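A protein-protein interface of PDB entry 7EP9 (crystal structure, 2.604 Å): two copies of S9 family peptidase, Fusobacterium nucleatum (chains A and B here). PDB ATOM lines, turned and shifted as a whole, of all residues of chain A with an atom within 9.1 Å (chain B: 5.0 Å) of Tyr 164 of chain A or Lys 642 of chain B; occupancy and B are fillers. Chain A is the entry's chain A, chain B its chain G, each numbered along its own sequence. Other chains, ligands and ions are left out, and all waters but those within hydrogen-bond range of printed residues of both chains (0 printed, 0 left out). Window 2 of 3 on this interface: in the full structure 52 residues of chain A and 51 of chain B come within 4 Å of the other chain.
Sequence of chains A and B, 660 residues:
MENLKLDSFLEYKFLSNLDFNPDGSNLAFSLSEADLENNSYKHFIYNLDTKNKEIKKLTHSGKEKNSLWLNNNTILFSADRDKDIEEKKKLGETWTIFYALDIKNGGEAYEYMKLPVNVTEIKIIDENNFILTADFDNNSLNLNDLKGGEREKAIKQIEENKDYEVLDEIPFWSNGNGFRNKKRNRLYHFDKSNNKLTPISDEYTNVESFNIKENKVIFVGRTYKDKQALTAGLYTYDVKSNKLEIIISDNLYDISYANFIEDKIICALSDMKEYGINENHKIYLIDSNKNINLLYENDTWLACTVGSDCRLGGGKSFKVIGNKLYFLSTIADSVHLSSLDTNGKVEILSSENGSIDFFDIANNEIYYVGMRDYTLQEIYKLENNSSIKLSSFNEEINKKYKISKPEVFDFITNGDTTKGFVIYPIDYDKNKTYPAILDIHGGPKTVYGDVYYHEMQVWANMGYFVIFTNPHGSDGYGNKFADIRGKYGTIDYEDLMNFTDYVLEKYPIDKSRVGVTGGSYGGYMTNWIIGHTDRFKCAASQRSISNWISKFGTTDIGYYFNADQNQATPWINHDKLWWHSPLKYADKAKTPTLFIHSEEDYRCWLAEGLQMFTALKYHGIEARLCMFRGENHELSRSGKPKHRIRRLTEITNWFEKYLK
Of the 14 printed residues of chain B, 7 touch a printed residue of chain A. Hydrophobic or aromatic side chains of chain B that line the printed part of chain A: Met 627, Phe 628 and His 643. Of the 14 printed residues of chain A, 8 touch a printed residue of chain B. Hydrophobic or aromatic side chains of chain A that line the printed part of chain B: Tyr 164, Val 166 and Phe 179. Among the printed residues, Asp or Glu carboxylates within 4 Å of a Lys or Arg side-chain nitrogen of the other chain: Glu 160 of chain A with Lys 642 of chain B (3.1 Å) and Glu 165 of chain A with Arg 629 of chain B (2.6 Å).
Of chain B, only Met 627, Phe 628, Arg 629, Lys 642, His 643 and Arg 646 come within 4 Å of Tyr 164 of chain A. Of chain A, only Glu 160 and Tyr 164 come within 4 Å of Lys 642 of chain B. Pro 641 of chain B touches none of the printed residues of chain A. No residue of chain A comes within 4 Å of Ile 645 of chain B. Printed residues of chain B within 4 Å of Asp 163 of chain A: Met 627, Phe 628, Arg 629 and His 643. Printed residues of chain B within 4 Å of Lys 162 of chain A: Arg 629. Of the printed residues of chain A, Arg 646 of chain B touches Asn 161 (3.7 Å), Tyr 164 (3.2 Å) and Val 166 (3.4 Å). Of the printed residues of chain B, Val 166 of chain A touches Arg 646. Leu 167 of chain A touches none of the printed residues of chain B.
No position is printed for both chains. Of the 18 pairs that touch across the chains among the printed residues, none has its exchanged pair printed and touching as well.
NH1 of Arg 646 of chain B touches OD1 of Asn 161 of chain A, at 3.7 Å. O of Met 627 of chain B touches O of Asp 163 of chain A, at 3.8 Å. Asp 163 of chain A touches Phe 628 of chain B. Met 627 of chain B touches Tyr 164 of chain A. Phe 628 of chain B touches Tyr 164 of chain A. OH of Tyr 164 of chain A touches CD2 of His 643 of chain B, 3.0 Å away. Arg 646 of chain B touches Tyr 164 of chain A. O of Glu 165 of chain A touches CA of Cys 626 of chain B, at 3.6 Å. NH2 of Arg 646 of chain B touches CG2 of Val 166 of chain A, at 3.4 Å. NH2 of Arg 629 of chain B touches CE1 of Phe 179 of chain A (3.8 Å).
The backbone NH (N) of Met 627 of chain B is in hydrogen-bond range of the backbone carbonyl oxygen (O) of Glu 165 of chain A, 2.8 Å away. The guanidinium group (NH1) of Arg 629 of chain B lies within hydrogen-bond range of the backbone carbonyl oxygen (O) of Lys 162 of chain A (2.9 Å). N of Arg 629 of chain B lies within hydrogen-bond range of O of Asp 163 of chain A (2.9 Å). The backbone carbonyl oxygen of Tyr 164 of chain A lies within hydrogen-bond range of the guanidinium group of Arg 629 of chain B (3.2 Å). NH2 of Arg 629 of chain B lies within salt-bridge range of OE2 of Glu 165 of chain A (2.6 Å). NZ of Lys 642 of chain B lies within salt-bridge range of OE2 of Glu 160 of chain A. The backbone carbonyl oxygen of Lys 642 of chain B lies within hydrogen-bond range of the side-chain hydroxyl of Tyr 164 of chain A, at 3.4 Å. The side-chain carboxylate of Asp 163 of chain A sits at hydrogen-bond distance from a ring nitrogen (NE2) of His 643 of chain B.
N of Lys 642 of chain B is in hydrogen-bond range of OD1 of Asn 39 of chain B, 2.7 Å away. The backbone carbonyl oxygen (O) of Gln 157 of chain A lies within hydrogen-bond range of the side-chain amide nitrogen (ND2) of Asn 161 of chain A, at 3.2 Å. The side-chain carboxylate (OE1) of Glu 159 of chain A is in salt-bridge range of the side-chain amino group (NZ) of Lys 162 of chain A (2.9 Å).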
ATOM      1  N   LYS A 156     -14.689  14.997  -4.411  1.00  0.00           N
ATOM      2  CA  LYS A 156     -15.001  16.175  -3.610  1.00  0.00           C
ATOM      3  C   LYS A 156     -14.339  17.424  -4.180  1.00  0.00           C
ATOM      4  O   LYS A 156     -14.950  18.499  -4.208  1.00  0.00           O
ATOM      5  CB  LYS A 156     -14.572  15.948  -2.161  1.00  0.00           C
ATOM      6  CG  LYS A 156     -14.788  17.141  -1.246  1.00  0.00           C
ATOM      7  CD  LYS A 156     -14.775  16.710   0.211  1.00  0.00           C
ATOM      8  CE  LYS A 156     -14.282  17.826   1.116  1.00  0.00           C
ATOM      9  NZ  LYS A 156     -13.771  17.297   2.411  1.00  0.00           N
ATOM     10  N   GLN A 157     -13.092  17.303  -4.641  1.00  0.00           N
ATOM     11  CA  GLN A 157     -12.404  18.452  -5.223  1.00  0.00           C
ATOM     12  C   GLN A 157     -13.083  18.906  -6.508  1.00  0.00           C
ATOM     13  O   GLN A 157     -13.212  20.111  -6.758  1.00  0.00           O
ATOM     14  CB  GLN A 157     -10.936  18.110  -5.481  1.00  0.00           C
ATOM     15  CG  GLN A 157     -10.073  19.310  -5.840  1.00  0.00           C
ATOM     16  CD  GLN A 157      -9.747  20.179  -4.641  1.00  0.00           C
ATOM     17  OE1 GLN A 157      -9.879  21.401  -4.691  1.00  0.00           O
ATOM     18  NE2 GLN A 157      -9.317  19.549  -3.552  1.00  0.00           N
ATOM     19  N   ILE A 158     -13.522  17.957  -7.338  1.00  0.00           N
ATOM     20  CA  ILE A 158     -14.239  18.310  -8.561  1.00  0.00           C
ATOM     21  C   ILE A 158     -15.565  18.980  -8.223  1.00  0.00           C
ATOM     22  O   ILE A 158     -15.996  19.921  -8.902  1.00  0.00           O
ATOM     23  CB  ILE A 158     -14.437  17.062  -9.442  1.00  0.00           C
ATOM     24  CG1 ILE A 158     -13.092  16.565  -9.975  1.00  0.00           C
ATOM     25  CG2 ILE A 158     -15.380  17.355 -10.598  1.00  0.00           C
ATOM     26  CD1 ILE A 158     -13.158  15.199 -10.619  1.00  0.00           C
ATOM     27  N   GLU A 159     -16.226  18.516  -7.159  1.00  0.00           N
ATOM     28  CA  GLU A 159     -17.489  19.124  -6.752  1.00  0.00           C
ATOM     29  C   GLU A 159     -17.277  20.535  -6.214  1.00  0.00           C
ATOM     30  O   GLU A 159     -18.057  21.444  -6.520  1.00  0.00           O
ATOM     31  CB  GLU A 159     -18.179  18.246  -5.707  1.00  0.00           C
ATOM     32  CG  GLU A 159     -19.552  18.743  -5.281  1.00  0.00           C
ATOM     33  CD  GLU A 159     -20.552  18.749  -6.421  1.00  0.00           C
ATOM     34  OE1 GLU A 159     -20.464  17.866  -7.301  1.00  0.00           O
ATOM     35  OE2 GLU A 159     -21.430  19.638  -6.435  1.00  0.00           O
ATOM     36  N   GLU A 160     -16.227  20.736  -5.415  1.00  0.00           N
ATOM     37  CA  GLU A 160     -15.957  22.063  -4.869  1.00  0.00           C
ATOM     38  C   GLU A 160     -15.493  23.025  -5.955  1.00  0.00           C
ATOM     39  O   GLU A 160     -15.818  24.218  -5.914  1.00  0.00           O
ATOM     40  CB  GLU A 160     -14.911  21.976  -3.760  1.00  0.00           C
ATOM     41  CG  GLU A 160     -15.383  21.273  -2.501  1.00  0.00           C
ATOM     42  CD  GLU A 160     -14.323  21.267  -1.416  1.00  0.00           C
ATOM     43  OE1 GLU A 160     -13.232  21.829  -1.650  1.00  0.00           O
ATOM     44  OE2 GLU A 160     -14.581  20.702  -0.334  1.00  0.00           O
ATOM     45  N   ASN A 161     -14.732  22.529  -6.933  1.00  0.00           N
ATOM     46  CA  ASN A 161     -14.204  23.383  -7.990  1.00  0.00           C
ATOM     47  C   ASN A 161     -15.292  23.962  -8.884  1.00  0.00           C
ATOM     48  O   ASN A 161     -15.004  24.874  -9.666  1.00  0.00           O
ATOM     49  CB  ASN A 161     -13.196  22.606  -8.839  1.00  0.00           C
ATOM     50  CG  ASN A 161     -11.795  22.647  -8.261  1.00  0.00           C
ATOM     51  OD1 ASN A 161     -11.414  23.608  -7.593  1.00  0.00           O
ATOM     52  ND2 ASN A 161     -11.020  21.600  -8.516  1.00  0.00           N
ATOM     53  N   LYS A 162     -16.526  23.462  -8.789  1.00  0.00           N
ATOM     54  CA  LYS A 162     -17.637  24.046  -9.532  1.00  0.00           C
ATOM     55  C   LYS A 162     -18.006  25.438  -9.038  1.00  0.00           C
ATOM     56  O   LYS A 162     -18.735  26.150  -9.736  1.00  0.00           O
ATOM     57  CB  LYS A 162     -18.864  23.136  -9.452  1.00  0.00           C
ATOM     58  CG  LYS A 162     -18.683  21.779 -10.109  1.00  0.00           C
ATOM     59  CD  LYS A 162     -19.956  20.955 -10.016  1.00  0.00           C
ATOM     60  CE  LYS A 162     -19.692  19.490 -10.317  1.00  0.00           C
ATOM     61  NZ  LYS A 162     -20.878  18.642 -10.014  1.00  0.00           N
ATOM     62  N   ASP A 163     -17.530  25.839  -7.861  1.00  0.00           N
ATOM     63  CA  ASP A 163     -17.802  27.161  -7.317  1.00  0.00           C
ATOM     64  C   ASP A 163     -16.801  28.212  -7.778  1.00  0.00           C
ATOM     65  O   ASP A 163     -16.905  29.368  -7.357  1.00  0.00           O
ATOM     66  CB  ASP A 163     -17.813  27.113  -5.784  1.00  0.00           C
ATOM     67  CG  ASP A 163     -18.767  26.068  -5.235  1.00  0.00           C
ATOM     68  OD1 ASP A 163     -19.666  25.628  -5.982  1.00  0.00           O
ATOM     69  OD2 ASP A 163     -18.617  25.690  -4.055  1.00  0.00           O
ATOM     70  N   TYR A 164     -15.840  27.848  -8.625  1.00  0.00           N
ATOM     71  CA  TYR A 164     -14.809  28.782  -9.051  1.00  0.00           C
ATOM     72  C   TYR A 164     -14.554  28.655 -10.545  1.00  0.00           C
ATOM     73  O   TYR A 164     -14.923  27.668 -11.186  1.00  0.00           O
ATOM     74  CB  TYR A 164     -13.484  28.564  -8.309  1.00  0.00           C
ATOM     75  CG  TYR A 164     -13.617  28.301  -6.831  1.00  0.00           C
ATOM     76  CD1 TYR A 164     -13.892  29.332  -5.944  1.00  0.00           C
ATOM     77  CD2 TYR A 164     -13.448  27.023  -6.320  1.00  0.00           C
ATOM     78  CE1 TYR A 164     -14.008  29.095  -4.588  1.00  0.00           C
ATOM     79  CE2 TYR A 164     -13.559  26.775  -4.969  1.00  0.00           C
ATOM     80  CZ  TYR A 164     -13.838  27.813  -4.107  1.00  0.00           C
ATOM     81  OH  TYR A 164     -13.948  27.565  -2.758  1.00  0.00           O
ATOM     82  N   GLU A 165     -13.908  29.686 -11.087  1.00  0.00           N
ATOM     83  CA  GLU A 165     -13.303  29.657 -12.411  1.00  0.00           C
ATOM     84  C   GLU A 165     -11.986  30.411 -12.329  1.00  0.00           C
ATOM     85  O   GLU A 165     -11.949  31.545 -11.841  1.00  0.00           O
ATOM     86  CB  GLU A 165     -14.211  30.288 -13.477  1.00  0.00           C
ATOM     87  CG  GLU A 165     -15.565  29.616 -13.652  1.00  0.00           C
ATOM     88  CD  GLU A 165     -15.479  28.261 -14.335  1.00  0.00           C
ATOM     89  OE1 GLU A 165     -14.381  27.884 -14.798  1.00  0.00           O
ATOM     90  OE2 GLU A 165     -16.517  27.569 -14.409  1.00  0.00           O
ATOM     91  N   VAL A 166     -10.908  29.780 -12.787  1.00  0.00           N
ATOM     92  CA  VAL A 166      -9.573  30.368 -12.765  1.00  0.00           C
ATOM     93  C   VAL A 166      -9.205  30.761 -14.187  1.00  0.00           C
ATOM     94  O   VAL A 166      -9.399  29.977 -15.123  1.00  0.00           O
ATOM     95  CB  VAL A 166      -8.539  29.394 -12.170  1.00  0.00           C
ATOM     96  CG1 VAL A 166      -7.132  29.952 -12.314  1.00  0.00           C
ATOM     97  CG2 VAL A 166      -8.857  29.114 -10.710  1.00  0.00           C
ATOM     98  N   LEU A 167      -8.685  31.977 -14.352  1.00  0.00           N
ATOM     99  CA  LEU A 167      -8.352  32.515 -15.665  1.00  0.00           C
ATOM    100  C   LEU A 167      -6.899  32.964 -15.684  1.00  0.00           C
ATOM    101  O   LEU A 167      -6.467  33.718 -14.806  1.00  0.00           O
ATOM    102  CB  LEU A 167      -9.262  33.694 -16.031  1.00  0.00           C
ATOM    103  CG  LEU A 167     -10.750  33.612 -15.686  1.00  0.00           C
ATOM    104  CD1 LEU A 167     -11.468  34.871 -16.147  1.00  0.00           C
ATOM    105  CD2 LEU A 167     -11.395  32.378 -16.296  1.00  0.00           C
ATOM    106  N   PHE A 179     -16.689  28.244 -20.068  1.00  0.00           N
ATOM    107  CA  PHE A 179     -15.314  28.595 -19.734  1.00  0.00           C
ATOM    108  C   PHE A 179     -14.347  27.585 -20.341  1.00  0.00           C
ATOM    109  O   PHE A 179     -14.593  26.376 -20.323  1.00  0.00           O
ATOM    110  CB  PHE A 179     -15.132  28.652 -18.217  1.00  0.00           C
ATOM    111  CG  PHE A 179     -15.742  29.867 -17.576  1.00  0.00           C
ATOM    112  CD1 PHE A 179     -17.076  29.875 -17.201  1.00  0.00           C
ATOM    113  CD2 PHE A 179     -14.980  31.001 -17.344  1.00  0.00           C
ATOM    114  CE1 PHE A 179     -17.639  30.992 -16.610  1.00  0.00           C
ATOM    115  CE2 PHE A 179     -15.537  32.119 -16.752  1.00  0.00           C
ATOM    116  CZ  PHE A 179     -16.869  32.115 -16.385  1.00  0.00           C
ATOM    117  N   LYS A 183      -8.046  24.685 -21.223  1.00  0.00           N
ATOM    118  CA  LYS A 183      -8.665  23.525 -21.843  1.00  0.00           C
ATOM    119  C   LYS A 183      -8.592  23.683 -23.354  1.00  0.00           C
ATOM    120  O   LYS A 183      -8.767  24.786 -23.882  1.00  0.00           O
ATOM    121  CB  LYS A 183     -10.118  23.360 -21.387  1.00  0.00           C
ATOM    122  CG  LYS A 183     -10.287  23.339 -19.874  1.00  0.00           C
ATOM    123  CD  LYS A 183     -11.751  23.252 -19.476  1.00  0.00           C
ATOM    124  CE  LYS A 183     -11.932  23.474 -17.982  1.00  0.00           C
ATOM    125  NZ  LYS A 183     -11.582  24.865 -17.576  1.00  0.00           N
ATOM    126  N   LEU B  36     -17.157  24.187   8.375  1.00  0.00           N
ATOM    127  CA  LEU B  36     -16.465  23.914   7.119  1.00  0.00           C
ATOM    128  C   LEU B  36     -17.081  22.732   6.380  1.00  0.00           C
ATOM    129  O   LEU B  36     -17.204  22.756   5.150  1.00  0.00           O
ATOM    130  CB  LEU B  36     -14.981  23.660   7.384  1.00  0.00           C
ATOM    131  CG  LEU B  36     -14.135  23.253   6.176  1.00  0.00           C
ATOM    132  CD1 LEU B  36     -13.871  24.455   5.286  1.00  0.00           C
ATOM    133  CD2 LEU B  36     -12.829  22.609   6.618  1.00  0.00           C
ATOM    134  N   GLU B  37     -17.475  21.688   7.116  1.00  0.00           N
ATOM    135  CA  GLU B  37     -17.974  20.476   6.472  1.00  0.00           C
ATOM    136  C   GLU B  37     -19.244  20.751   5.674  1.00  0.00           C
ATOM    137  O   GLU B  37     -19.460  20.157   4.612  1.00  0.00           O
ATOM    138  CB  GLU B  37     -18.220  19.390   7.518  1.00  0.00           C
ATOM    139  CG  GLU B  37     -18.071  17.974   6.985  1.00  0.00           C
ATOM    140  CD  GLU B  37     -19.327  17.478   6.295  1.00  0.00           C
ATOM    141  OE1 GLU B  37     -20.433  17.747   6.808  1.00  0.00           O
ATOM    142  OE2 GLU B  37     -19.208  16.820   5.240  1.00  0.00           O
ATOM    143  N   ASN B  39     -19.955  23.936   4.710  1.00  0.00           N
ATOM    144  CA  ASN B  39     -19.672  25.189   4.008  1.00  0.00           C
ATOM    145  C   ASN B  39     -20.720  26.250   4.334  1.00  0.00           C
ATOM    146  O   ASN B  39     -21.273  26.912   3.452  1.00  0.00           O
ATOM    147  CB  ASN B  39     -19.568  24.961   2.499  1.00  0.00           C
ATOM    148  CG  ASN B  39     -18.722  26.013   1.810  1.00  0.00           C
ATOM    149  OD1 ASN B  39     -17.906  26.681   2.446  1.00  0.00           O
ATOM    150  ND2 ASN B  39     -18.912  26.167   0.504  1.00  0.00           N
ATOM    151  N   CYS B 626      -9.480  34.740 -10.212  1.00  0.00           N
ATOM    152  CA  CYS B 626     -10.281  33.711  -9.565  1.00  0.00           C
ATOM    153  C   CYS B 626     -11.693  34.246  -9.380  1.00  0.00           C
ATOM    154  O   CYS B 626     -11.901  35.228  -8.659  1.00  0.00           O
ATOM    155  CB  CYS B 626      -9.676  33.296  -8.223  1.00  0.00           C
ATOM    156  SG  CYS B 626     -10.302  31.723  -7.594  1.00  0.00           S
ATOM    157  N   MET B 627     -12.654  33.607 -10.037  1.00  0.00           N
ATOM    158  CA  MET B 627     -14.052  34.002  -9.977  1.00  0.00           C
ATOM    159  C   MET B 627     -14.793  33.110  -8.990  1.00  0.00           C
ATOM    160  O   MET B 627     -14.613  31.890  -8.986  1.00  0.00           O
ATOM    161  CB  MET B 627     -14.691  33.913 -11.364  1.00  0.00           C
ATOM    162  CG  MET B 627     -16.155  34.294 -11.420  1.00  0.00           C
ATOM    163  SD  MET B 627     -16.679  34.536 -13.126  1.00  0.00           S
ATOM    164  CE  MET B 627     -18.423  34.172 -12.999  1.00  0.00           C
ATOM    165  N   PHE B 628     -15.619  33.724  -8.148  1.00  0.00           N
ATOM    166  CA  PHE B 628     -16.317  33.023  -7.078  1.00  0.00           C
ATOM    167  C   PHE B 628     -17.814  33.027  -7.358  1.00  0.00           C
ATOM    168  O   PHE B 628     -18.423  34.094  -7.487  1.00  0.00           O
ATOM    169  CB  PHE B 628     -16.026  33.666  -5.721  1.00  0.00           C
ATOM    170  CG  PHE B 628     -14.612  33.476  -5.249  1.00  0.00           C
ATOM    171  CD1 PHE B 628     -13.575  34.198  -5.816  1.00  0.00           C
ATOM    172  CD2 PHE B 628     -14.320  32.578  -4.236  1.00  0.00           C
ATOM    173  CE1 PHE B 628     -12.276  34.026  -5.385  1.00  0.00           C
ATOM    174  CE2 PHE B 628     -13.022  32.401  -3.799  1.00  0.00           C
ATOM    175  CZ  PHE B 628     -11.998  33.127  -4.374  1.00  0.00           C
ATOM    176  N   ARG B 629     -18.399  31.836  -7.451  1.00  0.00           N
ATOM    177  CA  ARG B 629     -19.838  31.688  -7.600  1.00  0.00           C
ATOM    178  C   ARG B 629     -20.508  31.688  -6.232  1.00  0.00           C
ATOM    179  O   ARG B 629     -19.939  31.227  -5.239  1.00  0.00           O
ATOM    180  CB  ARG B 629     -20.181  30.398  -8.344  1.00  0.00           C
ATOM    181  CG  ARG B 629     -19.891  30.429  -9.834  1.00  0.00           C
ATOM    182  CD  ARG B 629     -20.331  29.133 -10.499  1.00  0.00           C
ATOM    183  NE  ARG B 629     -20.053  29.128 -11.932  1.00  0.00           N
ATOM    184  CZ  ARG B 629     -18.951  28.623 -12.476  1.00  0.00           C
ATOM    185  NH1 ARG B 629     -18.017  28.082 -11.705  1.00  0.00           N
ATOM    186  NH2 ARG B 629     -18.781  28.661 -13.790  1.00  0.00           N
ATOM    187  N   LYS B 640     -18.968  32.079   2.420  1.00  0.00           N
ATOM    188  CA  LYS B 640     -18.968  30.714   2.919  1.00  0.00           C
ATOM    189  C   LYS B 640     -17.540  30.269   3.244  1.00  0.00           C
ATOM    190  O   LYS B 640     -16.582  30.732   2.620  1.00  0.00           O
ATOM    191  CB  LYS B 640     -19.608  29.776   1.897  1.00  0.00           C
ATOM    192  CG  LYS B 640     -21.093  30.052   1.685  1.00  0.00           C
ATOM    193  CD  LYS B 640     -21.727  29.070   0.715  1.00  0.00           C
ATOM    194  CE  LYS B 640     -23.159  29.473   0.397  1.00  0.00           C
ATOM    195  NZ  LYS B 640     -23.239  30.875  -0.105  1.00  0.00           N
ATOM    196  N   PRO B 641     -17.378  29.380   4.233  1.00  0.00           N
ATOM    197  CA  PRO B 641     -16.020  29.084   4.741  1.00  0.00           C
ATOM    198  C   PRO B 641     -15.027  28.645   3.677  1.00  0.00           C
ATOM    199  O   PRO B 641     -13.901  29.161   3.639  1.00  0.00           O
ATOM    200  CB  PRO B 641     -16.260  27.972   5.776  1.00  0.00           C
ATOM    201  CG  PRO B 641     -17.731  27.876   5.980  1.00  0.00           C
ATOM    202  CD  PRO B 641     -18.441  28.849   5.101  1.00  0.00           C
ATOM    203  N   LYS B 642     -15.400  27.695   2.816  1.00  0.00           N
ATOM    204  CA  LYS B 642     -14.459  27.197   1.818  1.00  0.00           C
ATOM    205  C   LYS B 642     -14.061  28.292   0.836  1.00  0.00           C
ATOM    206  O   LYS B 642     -12.909  28.347   0.388  1.00  0.00           O
ATOM    207  CB  LYS B 642     -15.058  26.003   1.075  1.00  0.00           C
ATOM    208  CG  LYS B 642     -15.069  24.716   1.880  1.00  0.00           C
ATOM    209  CD  LYS B 642     -15.911  23.647   1.207  1.00  0.00           C
ATOM    210  CE  LYS B 642     -15.994  22.395   2.063  1.00  0.00           C
ATOM    211  NZ  LYS B 642     -16.960  21.409   1.506  1.00  0.00           N
ATOM    212  N   HIS B 643     -14.999  29.175   0.494  1.00  0.00           N
ATOM    213  CA  HIS B 643     -14.688  30.255  -0.435  1.00  0.00           C
ATOM    214  C   HIS B 643     -13.845  31.337   0.230  1.00  0.00           C
ATOM    215  O   HIS B 643     -13.023  31.976  -0.437  1.00  0.00           O
ATOM    216  CB  HIS B 643     -15.980  30.834  -1.005  1.00  0.00           C
ATOM    217  CG  HIS B 643     -16.913  29.796  -1.547  1.00  0.00           C
ATOM    218  ND1 HIS B 643     -18.283  29.957  -1.562  1.00  0.00           N
ATOM    219  CD2 HIS B 643     -16.673  28.579  -2.090  1.00  0.00           C
ATOM    220  CE1 HIS B 643     -18.844  28.885  -2.091  1.00  0.00           C
ATOM    221  NE2 HIS B 643     -17.889  28.034  -2.421  1.00  0.00           N
ATOM    222  N   ARG B 644     -14.030  31.554   1.535  1.00  0.00           N
ATOM    223  CA  ARG B 644     -13.130  32.441   2.264  1.00  0.00           C
ATOM    224  C   ARG B 644     -11.722  31.865   2.315  1.00  0.00           C
ATOM    225  O   ARG B 644     -10.737  32.610   2.257  1.00  0.00           O
ATOM    226  CB  ARG B 644     -13.653  32.683   3.678  1.00  0.00           C
ATOM    227  CG  ARG B 644     -14.971  33.424   3.740  1.00  0.00           C
ATOM    228  CD  ARG B 644     -15.355  33.715   5.177  1.00  0.00           C
ATOM    229  NE  ARG B 644     -14.644  34.866   5.724  1.00  0.00           N
ATOM    230  CZ  ARG B 644     -15.032  35.535   6.804  1.00  0.00           C
ATOM    231  NH1 ARG B 644     -16.127  35.166   7.456  1.00  0.00           N
ATOM    232  NH2 ARG B 644     -14.326  36.571   7.233  1.00  0.00           N
ATOM    233  N   ILE B 645     -11.610  30.541   2.429  1.00  0.00           N
ATOM    234  CA  ILE B 645     -10.299  29.902   2.426  1.00  0.00           C
ATOM    235  C   ILE B 645      -9.684  29.964   1.034  1.00  0.00           C
ATOM    236  O   ILE B 645      -8.471  30.154   0.884  1.00  0.00           O
ATOM    237  CB  ILE B 645     -10.414  28.457   2.947  1.00  0.00           C
ATOM    238  CG1 ILE B 645     -10.504  28.455   4.475  1.00  0.00           C
ATOM    239  CG2 ILE B 645      -9.237  27.609   2.484  1.00  0.00           C
ATOM    240  CD1 ILE B 645     -10.952  27.136   5.063  1.00  0.00           C
ATOM    241  N   ARG B 646     -10.509  29.828  -0.008  1.00  0.00           N
ATOM    242  CA  ARG B 646      -9.997  29.905  -1.371  1.00  0.00           C
ATOM    243  C   ARG B 646      -9.474  31.302  -1.685  1.00  0.00           C
ATOM    244  O   ARG B 646      -8.394  31.453  -2.268  1.00  0.00           O
ATOM    245  CB  ARG B 646     -11.082  29.498  -2.368  1.00  0.00           C
ATOM    246  CG  ARG B 646     -10.614  29.489  -3.814  1.00  0.00           C
ATOM    247  CD  ARG B 646      -9.449  28.531  -4.013  1.00  0.00           C
ATOM    248  NE  ARG B 646      -8.950  28.554  -5.386  1.00  0.00           N
ATOM    249  CZ  ARG B 646      -9.365  27.733  -6.346  1.00  0.00           C
ATOM    250  NH1 ARG B 646     -10.289  26.819  -6.085  1.00  0.00           N
ATOM    251  NH2 ARG B 646      -8.856  27.824  -7.566  1.00  0.00           N
